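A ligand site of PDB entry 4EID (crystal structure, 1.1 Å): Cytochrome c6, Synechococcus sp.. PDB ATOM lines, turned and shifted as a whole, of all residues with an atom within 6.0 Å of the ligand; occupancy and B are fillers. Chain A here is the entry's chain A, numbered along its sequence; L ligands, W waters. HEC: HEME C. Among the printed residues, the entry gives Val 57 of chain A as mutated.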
ATOM      1  N   VAL A   9      -0.696 -17.960   5.690  1.00  0.00           N
ATOM      2  CA  VAL A   9       0.345 -17.552   4.788  1.00  0.00           C
ATOM      3  C   VAL A   9      -0.191 -17.357   3.404  1.00  0.00           C
ATOM      4  O   VAL A   9       0.109 -16.384   2.703  1.00  0.00           O
ATOM      5  CB  VAL A   9       1.584 -18.531   4.799  1.00  0.00           C
ATOM      6  CG1 VAL A   9       2.669 -17.984   3.875  1.00  0.00           C
ATOM      7  CG2 VAL A   9       2.100 -18.732   6.224  1.00  0.00           C
ATOM      8  N   PHE A  10      -0.979 -18.327   2.961  1.00  0.00           N
ATOM      9  CA  PHE A  10      -1.610 -18.311   1.654  1.00  0.00           C
ATOM     10  C   PHE A  10      -2.487 -17.056   1.495  1.00  0.00           C
ATOM     11  O   PHE A  10      -2.434 -16.347   0.512  1.00  0.00           O
ATOM     12  CB  PHE A  10      -2.440 -19.586   1.415  1.00  0.00           C
ATOM     13  CG  PHE A  10      -3.066 -19.629   0.064  1.00  0.00           C
ATOM     14  CD1 PHE A  10      -4.307 -19.119  -0.174  1.00  0.00           C
ATOM     15  CD2 PHE A  10      -2.367 -20.218  -0.995  1.00  0.00           C
ATOM     16  CE1 PHE A  10      -4.882 -19.178  -1.440  1.00  0.00           C
ATOM     17  CE2 PHE A  10      -2.930 -20.269  -2.259  1.00  0.00           C
ATOM     18  CZ  PHE A  10      -4.159 -19.759  -2.479  1.00  0.00           C
ATOM     19  N   ASN A  13      -0.300 -13.968   1.032  1.00  0.00           N
ATOM     20  CA  ASN A  13       0.786 -13.904   0.059  1.00  0.00           C
ATOM     21  C   ASN A  13       0.468 -14.492  -1.296  1.00  0.00           C
ATOM     22  O   ASN A  13       1.279 -14.367  -2.201  1.00  0.00           O
ATOM     23  CB  ASN A  13       2.041 -14.555   0.591  1.00  0.00           C
ATOM     24  CG  ASN A  13       2.570 -13.898   1.806  1.00  0.00           C
ATOM     25  OD1 ASN A  13       3.238 -12.861   1.695  1.00  0.00           O
ATOM     26  ND2 ASN A  13       2.240 -14.403   2.965  1.00  0.00           N
ATOM     27  N   CYS A  14      -0.653 -15.208  -1.417  1.00  0.00           N
ATOM     28  CA  CYS A  14      -0.842 -16.071  -2.579  1.00  0.00           C
ATOM     29  C   CYS A  14      -2.218 -16.005  -3.222  1.00  0.00           C
ATOM     30  O   CYS A  14      -2.405 -16.448  -4.349  1.00  0.00           O
ATOM     31  CB  CYS A  14      -0.573 -17.572  -2.228  1.00  0.00           C
ATOM     32  SG  CYS A  14       0.809 -17.878  -1.171  1.00  0.00           S
ATOM     33  N   ALA A  15      -3.188 -15.441  -2.518  1.00  0.00           N
ATOM     34  CA  ALA A  15      -4.549 -15.455  -2.987  1.00  0.00           C
ATOM     35  C   ALA A  15      -4.817 -14.491  -4.106  1.00  0.00           C
ATOM     36  O   ALA A  15      -5.736 -14.666  -4.874  1.00  0.00           O
ATOM     37  CB  ALA A  15      -5.536 -15.308  -1.849  1.00  0.00           C
ATOM     38  N   ALA A  16      -4.030 -13.408  -4.209  1.00  0.00           N
ATOM     39  CA  ALA A  16      -4.270 -12.486  -5.317  1.00  0.00           C
ATOM     40  C   ALA A  16      -4.035 -13.179  -6.674  1.00  0.00           C
ATOM     41  O   ALA A  16      -4.751 -12.959  -7.639  1.00  0.00           O
ATOM     42  CB  ALA A  16      -3.439 -11.196  -5.195  1.00  0.00           C
ATOM     43  N   CYS A  17      -3.030 -14.041  -6.748  1.00  0.00           N
ATOM     44  CA  CYS A  17      -2.747 -14.807  -7.954  1.00  0.00           C
ATOM     45  C   CYS A  17      -3.374 -16.194  -8.027  1.00  0.00           C
ATOM     46  O   CYS A  17      -3.517 -16.713  -9.131  1.00  0.00           O
ATOM     47  CB  CYS A  17      -1.244 -14.974  -8.125  1.00  0.00           C
ATOM     48  SG  CYS A  17      -0.435 -13.363  -8.432  1.00  0.00           S
ATOM     49  N   HIS A  18      -3.714 -16.754  -6.880  1.00  0.00           N
ATOM     50  CA  HIS A  18      -4.166 -18.161  -6.817  1.00  0.00           C
ATOM     51  C   HIS A  18      -5.444 -18.355  -6.046  1.00  0.00           C
ATOM     52  O   HIS A  18      -5.711 -19.389  -5.457  1.00  0.00           O
ATOM     53  CB  HIS A  18      -3.090 -19.064  -6.206  1.00  0.00           C
ATOM     54  CG  HIS A  18      -1.818 -19.167  -6.983  1.00  0.00           C
ATOM     55  ND1 HIS A  18      -1.743 -19.868  -8.164  1.00  0.00           N
ATOM     56  CD2 HIS A  18      -0.553 -18.847  -6.667  1.00  0.00           C
ATOM     57  CE1 HIS A  18      -0.492 -19.886  -8.561  1.00  0.00           C
ATOM     58  NE2 HIS A  18       0.265 -19.302  -7.642  1.00  0.00           N
ATOM     59  N   ASN A  23      -5.205 -20.176 -11.016  1.00  0.00           N
ATOM     60  CA  ASN A  23      -4.063 -19.388 -11.387  1.00  0.00           C
ATOM     61  C   ASN A  23      -4.508 -18.304 -12.334  1.00  0.00           C
ATOM     62  O   ASN A  23      -4.790 -18.589 -13.480  1.00  0.00           O
ATOM     63  CB  ASN A  23      -2.961 -20.298 -11.934  1.00  0.00           C
ATOM     64  CG  ASN A  23      -1.629 -19.572 -12.179  1.00  0.00           C
ATOM     65  OD1 ASN A  23      -1.616 -18.350 -12.476  1.00  0.00           O
ATOM     66  ND2 ASN A  23      -0.537 -20.273 -12.049  1.00  0.00           N
ATOM     67  N   VAL A  25      -2.946 -15.863 -13.672  1.00  0.00           N
ATOM     68  CA  VAL A  25      -1.944 -15.474 -14.671  1.00  0.00           C
ATOM     69  C   VAL A  25      -1.742 -16.542 -15.745  1.00  0.00           C
ATOM     70  O   VAL A  25      -1.703 -16.236 -16.952  1.00  0.00           O
ATOM     71  CB  VAL A  25      -0.559 -15.178 -14.000  1.00  0.00           C
ATOM     72  CG1 VAL A  25       0.538 -15.085 -15.038  1.00  0.00           C
ATOM     73  CG2 VAL A  25      -0.604 -13.901 -13.190  1.00  0.00           C
ATOM     74  N   MET A  26      -1.654 -17.804 -15.335  1.00  0.00           N
ATOM     75  CA  MET A  26      -1.428 -18.929 -16.215  1.00  0.00           C
ATOM     76  C   MET A  26      -2.474 -19.986 -15.873  1.00  0.00           C
ATOM     77  O   MET A  26      -2.236 -20.844 -15.029  1.00  0.00           O
ATOM     78  CB  MET A  26      -0.079 -19.518 -16.041  1.00  0.00           C
ATOM     79  CG  MET A  26       0.316 -20.471 -17.141  1.00  0.00           C
ATOM     80  SD  MET A  26       2.022 -20.936 -17.147  1.00  0.00           S
ATOM     81  CE  MET A  26       2.736 -19.405 -17.295  1.00  0.00           C
ATOM     82  N   THR A  28      -3.747 -22.745 -16.743  1.00  0.00           N
ATOM     83  CA  THR A  28      -3.564 -24.205 -16.711  1.00  0.00           C
ATOM     84  C   THR A  28      -2.832 -24.620 -15.446  1.00  0.00           C
ATOM     85  O   THR A  28      -2.969 -25.745 -14.980  1.00  0.00           O
ATOM     86  CB  THR A  28      -2.791 -24.728 -17.908  1.00  0.00           C
ATOM     87  OG1 THR A  28      -1.521 -24.053 -17.991  1.00  0.00           O
ATOM     88  CG2 THR A  28      -3.603 -24.564 -19.217  1.00  0.00           C
ATOM     89  N   LYS A  29      -2.007 -23.763 -14.913  1.00  0.00           N
ATOM     90  CA  LYS A  29      -1.067 -24.159 -13.859  1.00  0.00           C
ATOM     91  C   LYS A  29      -1.632 -23.863 -12.467  1.00  0.00           C
ATOM     92  O   LYS A  29      -1.149 -23.057 -11.677  1.00  0.00           O
ATOM     93  CB  LYS A  29       0.287 -23.544 -14.085  1.00  0.00           C
ATOM     94  CG  LYS A  29       0.921 -24.076 -15.447  1.00  0.00           C
ATOM     95  CD  LYS A  29       2.393 -23.999 -15.451  1.00  0.00           C
ATOM     96  CE  LYS A  29       2.972 -24.278 -16.783  1.00  0.00           C
ATOM     97  NZ  LYS A  29       4.472 -24.132 -16.729  1.00  0.00           N
ATOM     98  N   THR A  30      -2.709 -24.549 -12.185  1.00  0.00           N
ATOM     99  CA  THR A  30      -3.443 -24.376 -10.945  1.00  0.00           C
ATOM    100  C   THR A  30      -2.771 -25.161  -9.819  1.00  0.00           C
ATOM    101  O   THR A  30      -1.748 -25.834  -9.970  1.00  0.00           O
ATOM    102  CB  THR A  30      -4.925 -24.795 -11.034  1.00  0.00           C
ATOM    103  OG1 THR A  30      -4.884 -26.221 -11.140  1.00  0.00           O
ATOM    104  CG2 THR A  30      -5.587 -24.189 -12.250  1.00  0.00           C
ATOM    105  N   LEU A  31      -3.348 -25.014  -8.628  1.00  0.00           N
ATOM    106  CA  LEU A  31      -2.876 -25.662  -7.447  1.00  0.00           C
ATOM    107  C   LEU A  31      -3.688 -26.955  -7.157  1.00  0.00           C
ATOM    108  O   LEU A  31      -3.602 -27.452  -6.058  1.00  0.00           O
ATOM    109  CB  LEU A  31      -2.921 -24.690  -6.232  1.00  0.00           C
ATOM    110  CG  LEU A  31      -2.247 -23.334  -6.523  1.00  0.00           C
ATOM    111  CD1 LEU A  31      -2.159 -22.516  -5.234  1.00  0.00           C
ATOM    112  CD2 LEU A  31      -0.830 -23.485  -7.142  1.00  0.00           C
ATOM    113  N   LYS A  32      -4.474 -27.368  -8.140  1.00  0.00           N
ATOM    114  CA  LYS A  32      -5.191 -28.632  -7.988  1.00  0.00           C
ATOM    115  C   LYS A  32      -4.250 -29.799  -8.240  1.00  0.00           C
ATOM    116  O   LYS A  32      -3.253 -29.674  -8.936  1.00  0.00           O
ATOM    117  CB  LYS A  32      -6.378 -28.691  -8.926  1.00  0.00           C
ATOM    118  CG  LYS A  32      -7.576 -27.882  -8.404  1.00  0.00           C
ATOM    119  CD  LYS A  32      -7.420 -26.444  -8.262  1.00  0.00           C
ATOM    120  CE  LYS A  32      -8.779 -25.738  -7.977  1.00  0.00           C
ATOM    121  NZ  LYS A  32      -9.755 -25.657  -9.086  1.00  0.00           N
ATOM    122  N   ALA A  35      -3.214 -30.755 -11.926  1.00  0.00           N
ATOM    123  CA  ALA A  35      -2.341 -29.778 -12.552  1.00  0.00           C
ATOM    124  C   ALA A  35      -0.960 -29.802 -11.925  1.00  0.00           C
ATOM    125  O   ALA A  35       0.039 -29.753 -12.641  1.00  0.00           O
ATOM    126  CB  ALA A  35      -2.990 -28.373 -12.398  1.00  0.00           C
ATOM    127  N   LEU A  36      -0.849 -29.917 -10.610  1.00  0.00           N
ATOM    128  CA  LEU A  36       0.431 -29.909  -9.958  1.00  0.00           C
ATOM    129  C   LEU A  36       1.263 -31.083 -10.471  1.00  0.00           C
ATOM    130  O   LEU A  36       2.451 -30.937 -10.752  1.00  0.00           O
ATOM    131  CB  LEU A  36       0.274 -29.992  -8.469  1.00  0.00           C
ATOM    132  CG  LEU A  36      -0.294 -28.714  -7.818  1.00  0.00           C
ATOM    133  CD1 LEU A  36      -0.774 -29.025  -6.445  1.00  0.00           C
ATOM    134  CD2 LEU A  36       0.770 -27.625  -7.809  1.00  0.00           C
ATOM    135  N   TYR A  39       2.539 -30.240 -14.056  1.00  0.00           N
ATOM    136  CA  TYR A  39       3.317 -29.008 -14.341  1.00  0.00           C
ATOM    137  C   TYR A  39       4.378 -28.606 -13.325  1.00  0.00           C
ATOM    138  O   TYR A  39       5.278 -27.862 -13.700  1.00  0.00           O
ATOM    139  CB  TYR A  39       2.371 -27.833 -14.567  1.00  0.00           C
ATOM    140  CG  TYR A  39       1.429 -28.013 -15.702  1.00  0.00           C
ATOM    141  CD1 TYR A  39       1.887 -28.064 -17.017  1.00  0.00           C
ATOM    142  CD2 TYR A  39       0.086 -28.040 -15.501  1.00  0.00           C
ATOM    143  CE1 TYR A  39       1.013 -28.215 -18.064  1.00  0.00           C
ATOM    144  CE2 TYR A  39      -0.815 -28.174 -16.529  1.00  0.00           C
ATOM    145  CZ  TYR A  39      -0.342 -28.272 -17.836  1.00  0.00           C
ATOM    146  OH  TYR A  39      -1.194 -28.402 -18.883  1.00  0.00           O
ATOM    147  N   LEU A  40       4.253 -28.980 -12.065  1.00  0.00           N
ATOM    148  CA  LEU A  40       5.166 -28.443 -11.062  1.00  0.00           C
ATOM    149  C   LEU A  40       6.499 -29.140 -11.100  1.00  0.00           C
ATOM    150  O   LEU A  40       6.565 -30.353 -10.881  1.00  0.00           O
ATOM    151  CB  LEU A  40       4.531 -28.528  -9.703  1.00  0.00           C
ATOM    152  CG  LEU A  40       5.409 -28.111  -8.538  1.00  0.00           C
ATOM    153  CD1 LEU A  40       5.886 -26.634  -8.633  1.00  0.00           C
ATOM    154  CD2 LEU A  40       4.682 -28.305  -7.201  1.00  0.00           C
ATOM    155  N   ALA A  41       7.554 -28.370 -11.318  1.00  0.00           N
ATOM    156  CA  ALA A  41       8.905 -28.940 -11.381  1.00  0.00           C
ATOM    157  C   ALA A  41       9.196 -29.753 -10.135  1.00  0.00           C
ATOM    158  O   ALA A  41       8.812 -29.437  -9.044  1.00  0.00           O
ATOM    159  CB  ALA A  41       9.899 -27.828 -11.570  1.00  0.00           C
ATOM    160  N   ALA A  53       8.322 -29.680  -3.460  1.00  0.00           N
ATOM    161  CA  ALA A  53       8.303 -28.978  -4.688  1.00  0.00           C
ATOM    162  C   ALA A  53       7.611 -27.629  -4.539  1.00  0.00           C
ATOM    163  O   ALA A  53       8.014 -26.650  -5.198  1.00  0.00           O
ATOM    164  CB  ALA A  53       7.631 -29.797  -5.783  1.00  0.00           C
ATOM    165  N   VAL A  54       6.544 -27.566  -3.749  1.00  0.00           N
ATOM    166  CA  VAL A  54       5.891 -26.295  -3.481  1.00  0.00           C
ATOM    167  C   VAL A  54       6.834 -25.382  -2.696  1.00  0.00           C
ATOM    168  O   VAL A  54       6.931 -24.198  -3.043  1.00  0.00           O
ATOM    169  CB  VAL A  54       4.543 -26.471  -2.734  1.00  0.00           C
ATOM    170  CG1 VAL A  54       3.981 -25.090  -2.377  1.00  0.00           C
ATOM    171  CG2 VAL A  54       3.544 -27.271  -3.585  1.00  0.00           C
ATOM    172  N   VAL A  57       9.305 -23.837  -5.216  1.00  0.00           N
ATOM    173  CA  VAL A  57       8.775 -22.845  -6.082  1.00  0.00           C
ATOM    174  C   VAL A  57       8.410 -21.559  -5.317  1.00  0.00           C
ATOM    175  O   VAL A  57       8.607 -20.453  -5.845  1.00  0.00           O
ATOM    176  CB  VAL A  57       7.621 -23.325  -7.007  1.00  0.00           C
ATOM    177  CG1 VAL A  57       6.302 -23.511  -6.257  1.00  0.00           C
ATOM    178  CG2 VAL A  57       7.440 -22.411  -8.210  1.00  0.00           C
ATOM    179  N   VAL A  58       7.886 -21.677  -4.093  1.00  0.00           N
ATOM    180  CA  VAL A  58       7.667 -20.502  -3.276  1.00  0.00           C
ATOM    181  C   VAL A  58       8.972 -19.802  -2.987  1.00  0.00           C
ATOM    182  O   VAL A  58       9.065 -18.553  -3.058  1.00  0.00           O
ATOM    183  CB  VAL A  58       6.896 -20.904  -2.007  1.00  0.00           C
ATOM    184  CG1 VAL A  58       6.883 -19.710  -1.017  1.00  0.00           C
ATOM    185  CG2 VAL A  58       5.505 -21.300  -2.400  1.00  0.00           C
ATOM    186  N   GLN A  62       9.172 -18.960 -10.210  1.00  0.00           N
ATOM    187  CA  GLN A  62       9.159 -19.712 -11.479  1.00  0.00           C
ATOM    188  C   GLN A  62       8.454 -18.866 -12.493  1.00  0.00           C
ATOM    189  O   GLN A  62       7.290 -18.523 -12.301  1.00  0.00           O
ATOM    190  CB  GLN A  62       8.375 -21.041 -11.353  1.00  0.00           C
ATOM    191  CG  GLN A  62       8.088 -21.716 -12.670  1.00  0.00           C
ATOM    192  CD  GLN A  62       9.340 -22.037 -13.415  1.00  0.00           C
ATOM    193  OE1 GLN A  62      10.350 -22.392 -12.811  1.00  0.00           O
ATOM    194  NE2 GLN A  62       9.290 -21.884 -14.738  1.00  0.00           N
ATOM    195  N   GLY A  63       9.109 -18.538 -13.596  1.00  0.00           N
ATOM    196  CA  GLY A  63       8.421 -17.824 -14.642  1.00  0.00           C
ATOM    197  C   GLY A  63       7.928 -16.519 -14.105  1.00  0.00           C
ATOM    198  O   GLY A  63       8.702 -15.738 -13.560  1.00  0.00           O
ATOM    199  N   ALA A  64       6.658 -16.248 -14.294  1.00  0.00           N
ATOM    200  CA  ALA A  64       6.006 -15.025 -13.811  1.00  0.00           C
ATOM    201  C   ALA A  64       5.802 -14.994 -12.301  1.00  0.00           C
ATOM    202  O   ALA A  64       5.488 -13.947 -11.743  1.00  0.00           O
ATOM    203  CB  ALA A  64       4.683 -14.818 -14.548  1.00  0.00           C
ATOM    204  N   MET A  65       5.903 -16.149 -11.650  1.00  0.00           N
ATOM    205  CA  MET A  65       5.675 -16.191 -10.212  1.00  0.00           C
ATOM    206  C   MET A  65       6.903 -15.679  -9.454  1.00  0.00           C
ATOM    207  O   MET A  65       8.007 -16.144  -9.679  1.00  0.00           O
ATOM    208  CB  MET A  65       5.406 -17.605  -9.736  1.00  0.00           C
ATOM    209  CG  MET A  65       5.257 -17.692  -8.235  1.00  0.00           C
ATOM    210  SD  MET A  65       4.597 -19.262  -7.723  1.00  0.00           S
ATOM    211  CE  MET A  65       5.232 -19.322  -6.127  1.00  0.00           C
ATOM    212  N   PRO A  66       6.731 -14.648  -8.613  1.00  0.00           N
ATOM    213  CA  PRO A  66       7.890 -14.149  -7.834  1.00  0.00           C
ATOM    214  C   PRO A  66       8.411 -15.159  -6.846  1.00  0.00           C
ATOM    215  O   PRO A  66       7.683 -16.031  -6.370  1.00  0.00           O
ATOM    216  CB  PRO A  66       7.367 -12.869  -7.171  1.00  0.00           C
ATOM    217  CG  PRO A  66       6.009 -12.940  -7.196  1.00  0.00           C
ATOM    218  CD  PRO A  66       5.546 -13.872  -8.327  1.00  0.00           C
ATOM    219  N   PHE A  68       9.803 -15.841  -3.062  1.00  0.00           N
ATOM    220  CA  PHE A  68       9.522 -15.415  -1.706  1.00  0.00           C
ATOM    221  C   PHE A  68      10.680 -15.616  -0.744  1.00  0.00           C
ATOM    222  O   PHE A  68      10.581 -15.203   0.409  1.00  0.00           O
ATOM    223  CB  PHE A  68       8.258 -16.052  -1.148  1.00  0.00           C
ATOM    224  CG  PHE A  68       7.031 -15.571  -1.864  1.00  0.00           C
ATOM    225  CD1 PHE A  68       6.627 -16.100  -3.076  1.00  0.00           C
ATOM    226  CD2 PHE A  68       6.233 -14.566  -1.317  1.00  0.00           C
ATOM    227  CE1 PHE A  68       5.529 -15.601  -3.746  1.00  0.00           C
ATOM    228  CE2 PHE A  68       5.147 -14.080  -1.973  1.00  0.00           C
ATOM    229  CZ  PHE A  68       4.752 -14.612  -3.174  1.00  0.00           C
ATOM    230  N   LEU A  72       9.602 -14.182   3.124  1.00  0.00           N
ATOM    231  CA  LEU A  72       8.845 -14.942   4.100  1.00  0.00           C
ATOM    232  C   LEU A  72       9.790 -15.752   4.938  1.00  0.00           C
ATOM    233  O   LEU A  72      10.854 -16.204   4.451  1.00  0.00           O
ATOM    234  CB  LEU A  72       7.866 -15.896   3.374  1.00  0.00           C
ATOM    235  CG  LEU A  72       6.703 -15.227   2.645  1.00  0.00           C
ATOM    236  CD1 LEU A  72       5.916 -16.362   1.911  1.00  0.00           C
ATOM    237  CD2 LEU A  72       5.834 -14.465   3.601  1.00  0.00           C
ATOM    238  N   VAL A  80       3.125 -22.881   4.235  1.00  0.00           N
ATOM    239  CA  VAL A  80       2.287 -22.700   3.035  1.00  0.00           C
ATOM    240  C   VAL A  80       2.444 -23.919   2.083  1.00  0.00           C
ATOM    241  O   VAL A  80       1.464 -24.266   1.460  1.00  0.00           O
ATOM    242  CB  VAL A  80       2.476 -21.313   2.332  1.00  0.00           C
ATOM    243  CG1 VAL A  80       3.789 -21.281   1.459  1.00  0.00           C
ATOM    244  CG2 VAL A  80       1.262 -20.924   1.574  1.00  0.00           C
ATOM    245  N   ALA A  81       3.631 -24.467   1.969  1.00  0.00           N
ATOM    246  CA  ALA A  81       3.804 -25.663   1.153  1.00  0.00           C
ATOM    247  C   ALA A  81       2.941 -26.795   1.661  1.00  0.00           C
ATOM    248  O   ALA A  81       2.312 -27.520   0.864  1.00  0.00           O
ATOM    249  CB  ALA A  81       5.270 -26.025   1.101  1.00  0.00           C
ATOM    250  N   ILE A  84      -0.684 -26.061   0.615  1.00  0.00           N
ATOM    251  CA  ILE A  84      -0.921 -26.439  -0.775  1.00  0.00           C
ATOM    252  C   ILE A  84      -1.059 -27.960  -0.915  1.00  0.00           C
ATOM    253  O   ILE A  84      -1.957 -28.436  -1.582  1.00  0.00           O
ATOM    254  CB  ILE A  84       0.134 -25.890  -1.723  1.00  0.00           C
ATOM    255  CG1 ILE A  84       0.238 -24.343  -1.659  1.00  0.00           C
ATOM    256  CG2 ILE A  84      -0.162 -26.317  -3.140  1.00  0.00           C
ATOM    257  CD1 ILE A  84      -1.112 -23.639  -1.801  1.00  0.00           C
HETATM  258 FE   HEC L   1       2.263 -19.216  -7.654  1.00  0.00          FE
HETATM  259  CHA HEC L   1       2.776 -21.520 -10.047  1.00  0.00           C
HETATM  260  CHB HEC L   1       2.183 -21.677  -5.302  1.00  0.00           C
HETATM  261  CHC HEC L   1       2.402 -16.846  -5.272  1.00  0.00           C
HETATM  262  CHD HEC L   1       1.737 -16.816 -10.039  1.00  0.00           C
HETATM  263  NA  HEC L   1       2.423 -21.153  -7.688  1.00  0.00           N
HETATM  264  C1A HEC L   1       2.608 -21.990  -8.806  1.00  0.00           C
HETATM  265  C2A HEC L   1       2.631 -23.381  -8.383  1.00  0.00           C
HETATM  266  C3A HEC L   1       2.511 -23.434  -7.078  1.00  0.00           C
HETATM  267  C4A HEC L   1       2.389 -22.051  -6.608  1.00  0.00           C
HETATM  268  CMA HEC L   1       2.520 -24.625  -6.127  1.00  0.00           C
HETATM  269  CAA HEC L   1       2.727 -24.524  -9.399  1.00  0.00           C
HETATM  270  CBA HEC L   1       1.401 -24.723 -10.101  1.00  0.00           C
HETATM  271  CGA HEC L   1       1.402 -25.762 -11.221  1.00  0.00           C
HETATM  272  O1A HEC L   1       2.473 -26.011 -11.762  1.00  0.00           O
HETATM  273  O2A HEC L   1       0.278 -26.287 -11.608  1.00  0.00           O
HETATM  274  NB  HEC L   1       2.260 -19.262  -5.657  1.00  0.00           N
HETATM  275  C1B HEC L   1       2.165 -20.329  -4.870  1.00  0.00           C
HETATM  276  C2B HEC L   1       2.137 -19.963  -3.490  1.00  0.00           C
HETATM  277  C3B HEC L   1       2.198 -18.596  -3.485  1.00  0.00           C
HETATM  278  C4B HEC L   1       2.292 -18.168  -4.842  1.00  0.00           C
HETATM  279  CMB HEC L   1       1.944 -20.899  -2.347  1.00  0.00           C
HETATM  280  CAB HEC L   1       2.272 -17.661  -2.236  1.00  0.00           C
HETATM  281  CBB HEC L   1       3.430 -17.841  -1.407  1.00  0.00           C
HETATM  282  NC  HEC L   1       2.136 -17.272  -7.644  1.00  0.00           N
HETATM  283  C1C HEC L   1       2.196 -16.422  -6.544  1.00  0.00           C
HETATM  284  C2C HEC L   1       2.010 -15.050  -6.940  1.00  0.00           C
HETATM  285  C3C HEC L   1       1.721 -15.046  -8.240  1.00  0.00           C
HETATM  286  C4C HEC L   1       1.847 -16.432  -8.723  1.00  0.00           C
HETATM  287  CMC HEC L   1       2.053 -13.850  -5.974  1.00  0.00           C
HETATM  288  CAC HEC L   1       1.280 -13.879  -9.123  1.00  0.00           C
HETATM  289  CBC HEC L   1       2.071 -12.705  -9.300  1.00  0.00           C
HETATM  290  ND  HEC L   1       2.283 -19.180  -9.668  1.00  0.00           N
HETATM  291  C1D HEC L   1       2.083 -18.096 -10.480  1.00  0.00           C
HETATM  292  C2D HEC L   1       2.288 -18.434 -11.848  1.00  0.00           C
HETATM  293  C3D HEC L   1       2.689 -19.818 -11.819  1.00  0.00           C
HETATM  294  C4D HEC L   1       2.623 -20.250 -10.477  1.00  0.00           C
HETATM  295  CMD HEC L   1       2.242 -17.521 -13.036  1.00  0.00           C
HETATM  296  CAD HEC L   1       3.064 -20.642 -13.016  1.00  0.00           C
HETATM  297  CBD HEC L   1       4.576 -20.789 -13.047  1.00  0.00           C
HETATM  298  CGD HEC L   1       4.954 -21.511 -14.350  1.00  0.00           C
HETATM  299  O1D HEC L   1       5.178 -20.832 -15.347  1.00  0.00           O
HETATM  300  O2D HEC L   1       5.024 -22.735 -14.323  1.00  0.00           O
HETATM  301  O   HOH W   1      -0.868 -13.502  -4.754  1.00  0.00           O
HETATM  302  O   HOH W   2       4.904 -24.405 -12.201  1.00  0.00           O
HETATM  303  O   HOH W   3       7.137 -21.640 -16.760  1.00  0.00           O
HETATM  304  O   HOH W   4       4.887 -18.131 -15.473  1.00  0.00           O
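O2D of the ligand is in salt-bridge range of NZ of Lys 29, 2.8 Å away. An oxygen (O1A) of the ligand lies within hydrogen-bond range of the backbone NH of Leu 40, at 3.5 Å. FE of the ligand is bound by NE2 of His 18 (2.0 Å). O of Thr 30 sits close to O2A of the ligand (2.6 Å). The side-chain sulfur of Cys 17 is covalently linked to a carbon (CAC) of the ligand (1.9 Å). An iron atom (FE) of the ligand is bound by the side-chain sulfur (SD) of Met 65 (2.3 Å). The side-chain sulfur (SG) of Cys 14 is bonded to a carbon (CAB) of the ligand, 1.8 Å away.
O of Val 9 is in hydrogen-bond range of ND2 of Asn 13 (2.9 Å). The backbone NH (N) of Val 25 lies within hydrogen-bond range of the side-chain amide oxygen (OD1) of Asn 23 (3.1 Å). N of Lys 32 lies within hydrogen-bond range of OG1 of Thr 30 (3.2 Å). The backbone carbonyl oxygen (O) of Val 58 lies within hydrogen-bond range of the backbone NH (N) of Phe 68. N of Met 26 lies within hydrogen-bond range of OD1 of Asn 23 (2.9 Å). The backbone carbonyl oxygen (O) of Lys 29 sits at hydrogen-bond distance from the side-chain amide nitrogen (ND2) of Asn 23.
An oxygen (O1D) of the ligand lies close to the side-chain sulfur (SD) of Met 26 (3.6 Å). Merely in contact with the ligand: Asn 13 (3.4 Å), Asn 23 (3.3 Å), Val 25 (3.6 Å), Leu 31 (3.3 Å), Ala 35 (3.6 Å), Leu 36 (3.8 Å), Tyr 39 (3.3 Å), Val 54 (3.8 Å), Val 57 (3.9 Å), Val 58 (3.6 Å), Gln 62 (3.6 Å), Ala 64 (3.9 Å), Pro 66 (3.8 Å), Phe 68 (3.7 Å), Val 80 (3.98 Å) and Ile 84 (3.9 Å). Within 4 Å of the ligand: Asn 13, Cys 14, Cys 17, His 18, Asn 23, Val 25, Met 26, Lys 29, Thr 30, Leu 31, Ala 35, Leu 36, Tyr 39, Leu 40, Val 54, Val 57, Val 58, Gln 62, Ala 64, Met 65, Pro 66, Phe 68, Val 80 and Ile 84.
Water W3 bridges O1D of the ligand (2.5 Å) and NE2 of Gln 62 (3.0 Å). Water W4 lies within hydrogen-bond range of an oxygen (O1D) of the ligand (2.7 Å) and the backbone NH of Ala 64 (2.8 Å).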
